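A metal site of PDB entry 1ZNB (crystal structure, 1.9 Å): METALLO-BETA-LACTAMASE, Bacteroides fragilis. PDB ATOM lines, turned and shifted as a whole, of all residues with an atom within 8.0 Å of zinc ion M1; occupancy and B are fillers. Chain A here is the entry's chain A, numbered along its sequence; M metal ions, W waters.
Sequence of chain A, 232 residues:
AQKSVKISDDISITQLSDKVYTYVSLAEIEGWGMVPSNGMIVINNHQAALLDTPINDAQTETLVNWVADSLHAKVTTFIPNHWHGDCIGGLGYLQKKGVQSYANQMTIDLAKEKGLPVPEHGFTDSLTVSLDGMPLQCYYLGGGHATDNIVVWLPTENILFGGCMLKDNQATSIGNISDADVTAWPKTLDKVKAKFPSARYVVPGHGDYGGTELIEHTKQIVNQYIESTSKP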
ATOM      1  N   ASP A  52       1.356 -12.854 -19.778  1.00  0.00           N
ATOM      2  CA  ASP A  52       2.794 -13.190 -19.823  1.00  0.00           C
ATOM      3  C   ASP A  52       3.484 -12.710 -18.539  1.00  0.00           C
ATOM      4  O   ASP A  52       3.121 -11.674 -17.951  1.00  0.00           O
ATOM      5  CB  ASP A  52       3.493 -12.522 -21.023  1.00  0.00           C
ATOM      6  CG  ASP A  52       3.432 -13.337 -22.297  1.00  0.00           C
ATOM      7  OD1 ASP A  52       2.557 -14.197 -22.411  1.00  0.00           O
ATOM      8  OD2 ASP A  52       4.277 -13.114 -23.188  1.00  0.00           O
ATOM      9  N   ASN A  81       1.411 -16.457 -23.582  1.00  0.00           N
ATOM     10  CA  ASN A  81       1.346 -16.489 -25.022  1.00  0.00           C
ATOM     11  C   ASN A  81       1.768 -17.851 -25.593  1.00  0.00           C
ATOM     12  O   ASN A  81       1.193 -18.345 -26.590  1.00  0.00           O
ATOM     13  CB  ASN A  81       2.198 -15.356 -25.607  1.00  0.00           C
ATOM     14  CG  ASN A  81       1.987 -15.215 -27.063  1.00  0.00           C
ATOM     15  OD1 ASN A  81       2.757 -15.783 -27.847  1.00  0.00           O
ATOM     16  ND2 ASN A  81       0.893 -14.520 -27.447  1.00  0.00           N
ATOM     17  N   HIS A  82       2.845 -18.400 -25.022  1.00  0.00           N
ATOM     18  CA  HIS A  82       3.348 -19.729 -25.382  1.00  0.00           C
ATOM     19  C   HIS A  82       4.216 -20.243 -24.219  1.00  0.00           C
ATOM     20  O   HIS A  82       4.214 -19.623 -23.127  1.00  0.00           O
ATOM     21  CB  HIS A  82       4.049 -19.742 -26.751  1.00  0.00           C
ATOM     22  CG  HIS A  82       5.104 -18.703 -26.918  1.00  0.00           C
ATOM     23  ND1 HIS A  82       4.840 -17.356 -27.077  1.00  0.00           N
ATOM     24  CD2 HIS A  82       6.451 -18.833 -26.943  1.00  0.00           C
ATOM     25  CE1 HIS A  82       5.981 -16.749 -27.179  1.00  0.00           C
ATOM     26  NE2 HIS A  82       6.967 -17.618 -27.095  1.00  0.00           N
ATOM     27  N   TRP A  83       4.885 -21.395 -24.384  1.00  0.00           N
ATOM     28  CA  TRP A  83       5.645 -22.011 -23.289  1.00  0.00           C
ATOM     29  C   TRP A  83       7.044 -21.420 -22.990  1.00  0.00           C
ATOM     30  O   TRP A  83       7.646 -21.804 -21.973  1.00  0.00           O
ATOM     31  CB  TRP A  83       5.757 -23.509 -23.515  1.00  0.00           C
ATOM     32  CG  TRP A  83       6.574 -23.844 -24.741  1.00  0.00           C
ATOM     33  CD1 TRP A  83       6.135 -23.931 -26.034  1.00  0.00           C
ATOM     34  CD2 TRP A  83       7.990 -24.088 -24.784  1.00  0.00           C
ATOM     35  NE1 TRP A  83       7.175 -24.215 -26.866  1.00  0.00           N
ATOM     36  CE2 TRP A  83       8.332 -24.311 -26.145  1.00  0.00           C
ATOM     37  CE3 TRP A  83       9.016 -24.120 -23.787  1.00  0.00           C
ATOM     38  CZ2 TRP A  83       9.663 -24.581 -26.569  1.00  0.00           C
ATOM     39  CZ3 TRP A  83      10.341 -24.378 -24.205  1.00  0.00           C
ATOM     40  CH2 TRP A  83      10.633 -24.605 -25.607  1.00  0.00           C
ATOM     41  N   HIS A  84       7.557 -20.523 -23.833  1.00  0.00           N
ATOM     42  CA  HIS A  84       8.873 -19.915 -23.560  1.00  0.00           C
ATOM     43  C   HIS A  84       8.941 -19.136 -22.225  1.00  0.00           C
ATOM     44  O   HIS A  84       7.903 -18.716 -21.690  1.00  0.00           O
ATOM     45  CB  HIS A  84       9.319 -19.017 -24.720  1.00  0.00           C
ATOM     46  CG  HIS A  84       9.770 -19.797 -25.906  1.00  0.00           C
ATOM     47  ND1 HIS A  84       9.863 -19.273 -27.171  1.00  0.00           N
ATOM     48  CD2 HIS A  84      10.176 -21.083 -26.005  1.00  0.00           C
ATOM     49  CE1 HIS A  84      10.310 -20.194 -28.004  1.00  0.00           C
ATOM     50  NE2 HIS A  84      10.510 -21.307 -27.321  1.00  0.00           N
ATOM     51  N   GLY A  85      10.170 -18.999 -21.706  1.00  0.00           N
ATOM     52  CA  GLY A  85      10.473 -18.288 -20.441  1.00  0.00           C
ATOM     53  C   GLY A  85       9.975 -16.847 -20.311  1.00  0.00           C
ATOM     54  O   GLY A  85       9.633 -16.405 -19.205  1.00  0.00           O
ATOM     55  N   ASP A  86       9.940 -16.110 -21.435  1.00  0.00           N
ATOM     56  CA  ASP A  86       9.421 -14.731 -21.474  1.00  0.00           C
ATOM     57  C   ASP A  86       7.842 -14.734 -21.506  1.00  0.00           C
ATOM     58  O   ASP A  86       7.203 -13.698 -21.709  1.00  0.00           O
ATOM     59  CB  ASP A  86      10.007 -13.906 -22.663  1.00  0.00           C
ATOM     60  CG  ASP A  86       9.847 -14.584 -24.029  1.00  0.00           C
ATOM     61  OD1 ASP A  86      10.100 -15.797 -24.207  1.00  0.00           O
ATOM     62  OD2 ASP A  86       9.435 -13.866 -24.947  1.00  0.00           O
ATOM     63  N   CYS A  87       7.239 -15.896 -21.252  1.00  0.00           N
ATOM     64  CA  CYS A  87       5.805 -16.017 -21.171  1.00  0.00           C
ATOM     65  C   CYS A  87       5.407 -16.665 -19.832  1.00  0.00           C
ATOM     66  O   CYS A  87       4.476 -16.179 -19.156  1.00  0.00           O
ATOM     67  CB  CYS A  87       5.212 -16.845 -22.310  1.00  0.00           C
ATOM     68  SG  CYS A  87       5.610 -16.268 -23.915  1.00  0.00           S
ATOM     69  N   HIS A 145       5.680 -18.056 -34.406  1.00  0.00           N
ATOM     70  CA  HIS A 145       6.925 -17.982 -33.648  1.00  0.00           C
ATOM     71  C   HIS A 145       7.156 -19.301 -32.805  1.00  0.00           C
ATOM     72  O   HIS A 145       8.280 -19.765 -32.640  1.00  0.00           O
ATOM     73  CB  HIS A 145       6.863 -16.765 -32.698  1.00  0.00           C
ATOM     74  CG  HIS A 145       7.822 -16.898 -31.552  1.00  0.00           C
ATOM     75  ND1 HIS A 145       9.155 -16.589 -31.671  1.00  0.00           N
ATOM     76  CD2 HIS A 145       7.640 -17.353 -30.304  1.00  0.00           C
ATOM     77  CE1 HIS A 145       9.762 -16.836 -30.530  1.00  0.00           C
ATOM     78  NE2 HIS A 145       8.867 -17.310 -29.685  1.00  0.00           N
ATOM     79  N   ALA A 146       6.069 -19.791 -32.207  1.00  0.00           N
ATOM     80  CA  ALA A 146       6.053 -21.052 -31.455  1.00  0.00           C
ATOM     81  C   ALA A 146       4.830 -21.836 -32.004  1.00  0.00           C
ATOM     82  O   ALA A 146       3.888 -21.242 -32.538  1.00  0.00           O
ATOM     83  CB  ALA A 146       5.929 -20.792 -29.912  1.00  0.00           C
ATOM     84  N   ASP A 148       2.591 -23.318 -30.385  1.00  0.00           N
ATOM     85  CA  ASP A 148       1.425 -23.102 -29.504  1.00  0.00           C
ATOM     86  C   ASP A 148       1.019 -21.614 -29.312  1.00  0.00           C
ATOM     87  O   ASP A 148       0.097 -21.354 -28.542  1.00  0.00           O
ATOM     88  CB  ASP A 148       1.717 -23.725 -28.126  1.00  0.00           C
ATOM     89  CG  ASP A 148       2.957 -23.108 -27.455  1.00  0.00           C
ATOM     90  OD1 ASP A 148       3.935 -22.881 -28.145  1.00  0.00           O
ATOM     91  OD2 ASP A 148       2.937 -22.795 -26.252  1.00  0.00           O
ATOM     92  N   ASN A 149       1.697 -20.660 -29.981  1.00  0.00           N
ATOM     93  CA  ASN A 149       1.372 -19.255 -29.788  1.00  0.00           C
ATOM     94  C   ASN A 149      -0.089 -18.857 -30.035  1.00  0.00           C
ATOM     95  O   ASN A 149      -0.735 -19.255 -31.051  1.00  0.00           O
ATOM     96  CB  ASN A 149       2.358 -18.288 -30.480  1.00  0.00           C
ATOM     97  CG  ASN A 149       2.520 -18.485 -32.010  1.00  0.00           C
ATOM     98  OD1 ASN A 149       3.538 -18.074 -32.567  1.00  0.00           O
ATOM     99  ND2 ASN A 149       1.491 -18.985 -32.681  1.00  0.00           N
ATOM    100  N   GLY A 163       1.720 -10.911 -28.917  1.00  0.00           N
ATOM    101  CA  GLY A 163       2.824 -11.725 -28.446  1.00  0.00           C
ATOM    102  C   GLY A 163       3.970 -11.895 -29.468  1.00  0.00           C
ATOM    103  O   GLY A 163       4.003 -11.173 -30.469  1.00  0.00           O
ATOM    104  N   CYS A 164       4.846 -12.871 -29.229  1.00  0.00           N
ATOM    105  CA  CYS A 164       6.065 -13.104 -30.028  1.00  0.00           C
ATOM    106  C   CYS A 164       5.883 -13.450 -31.502  1.00  0.00           C
ATOM    107  O   CYS A 164       6.821 -13.357 -32.271  1.00  0.00           O
ATOM    108  CB  CYS A 164       6.972 -14.075 -29.317  1.00  0.00           C
ATOM    109  SG  CYS A 164       7.365 -13.585 -27.623  1.00  0.00           S
ATOM    110  N   MET A 165       4.679 -13.843 -31.903  1.00  0.00           N
ATOM    111  CA  MET A 165       4.424 -14.102 -33.315  1.00  0.00           C
ATOM    112  C   MET A 165       4.502 -12.708 -34.067  1.00  0.00           C
ATOM    113  O   MET A 165       4.627 -12.642 -35.286  1.00  0.00           O
ATOM    114  CB  MET A 165       3.043 -14.707 -33.487  1.00  0.00           C
ATOM    115  CG  MET A 165       1.843 -13.671 -33.405  1.00  0.00           C
ATOM    116  SD  MET A 165       0.353 -14.433 -34.061  1.00  0.00           S
ATOM    117  CE  MET A 165       0.049 -15.711 -32.721  1.00  0.00           C
ATOM    118  N   ASN A 176      14.691 -16.244 -33.045  1.00  0.00           N
ATOM    119  CA  ASN A 176      14.702 -17.641 -32.605  1.00  0.00           C
ATOM    120  C   ASN A 176      13.582 -18.415 -33.265  1.00  0.00           C
ATOM    121  O   ASN A 176      12.439 -18.187 -32.954  1.00  0.00           O
ATOM    122  CB  ASN A 176      14.516 -17.655 -31.076  1.00  0.00           C
ATOM    123  CG  ASN A 176      14.302 -19.068 -30.528  1.00  0.00           C
ATOM    124  OD1 ASN A 176      14.801 -20.056 -31.101  1.00  0.00           O
ATOM    125  ND2 ASN A 176      13.579 -19.174 -29.400  1.00  0.00           N
ATOM    126  N   ASP A 179      11.588 -23.191 -32.203  1.00  0.00           N
ATOM    127  CA  ASP A 179      10.271 -23.766 -31.907  1.00  0.00           C
ATOM    128  C   ASP A 179       9.189 -23.275 -32.804  1.00  0.00           C
ATOM    129  O   ASP A 179       8.035 -23.475 -32.547  1.00  0.00           O
ATOM    130  CB  ASP A 179       9.920 -23.449 -30.433  1.00  0.00           C
ATOM    131  CG  ASP A 179      11.011 -23.971 -29.500  1.00  0.00           C
ATOM    132  OD1 ASP A 179      11.269 -25.192 -29.576  1.00  0.00           O
ATOM    133  OD2 ASP A 179      11.733 -23.182 -28.836  1.00  0.00           O
ATOM    134  N   GLY A 205       5.737  -9.441 -28.820  1.00  0.00           N
ATOM    135  CA  GLY A 205       6.408 -10.132 -27.729  1.00  0.00           C
ATOM    136  C   GLY A 205       7.626  -9.382 -27.186  1.00  0.00           C
ATOM    137  O   GLY A 205       7.958  -9.451 -25.990  1.00  0.00           O
ATOM    138  N   HIS A 206       8.298  -8.681 -28.090  1.00  0.00           N
ATOM    139  CA  HIS A 206       9.479  -7.865 -27.806  1.00  0.00           C
ATOM    140  C   HIS A 206       9.466  -6.560 -28.622  1.00  0.00           C
ATOM    141  O   HIS A 206       9.117  -6.555 -29.809  1.00  0.00           O
ATOM    142  CB  HIS A 206      10.739  -8.661 -28.147  1.00  0.00           C
ATOM    143  CG  HIS A 206      10.765 -10.039 -27.562  1.00  0.00           C
ATOM    144  ND1 HIS A 206      11.296 -10.306 -26.319  1.00  0.00           N
ATOM    145  CD2 HIS A 206      10.292 -11.208 -28.031  1.00  0.00           C
ATOM    146  CE1 HIS A 206      11.155 -11.590 -26.057  1.00  0.00           C
ATOM    147  NE2 HIS A 206      10.555 -12.158 -27.084  1.00  0.00           N
HETATM  148 ZN    ZN M   1       9.040 -17.419 -27.623  1.00  0.00          ZN
HETATM  149 ZN    ZN M   2       9.576 -14.020 -27.180  1.00  0.00          ZN
HETATM  150  O   HOH W   1      10.038 -16.007 -26.889  1.00  0.00           O
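Zinc ion M1 is bound by water W1, a ring nitrogen (NE2) of His 145, a ring nitrogen (ND1) of His 84 and a ring nitrogen (NE2) of His 82. Zinc ion M1 has four donor atoms within binding distance.
The backbone NH (N) of His 145 lies within hydrogen-bond range of the side-chain amide oxygen (OD1) of Asn 149 (2.8 Å). The side-chain carboxylate (OD2) of Asp 179 is in hydrogen-bond range of a ring nitrogen (NE2) of His 84, at 2.7 Å. A ring nitrogen (ND1) of His 82 sits close to the side-chain sulfur (SG) of Cys 87, at 3.4 Å. A ring nitrogen (ND1) of His 82 sits at hydrogen-bond distance from the side-chain amide oxygen of Asn 81 (2.7 Å).
OD1 of Asp 86 touches zinc ion M1, at 3.9 Å. Of the 19 residues printed, 4 come within 4 Å of zinc ion M1.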
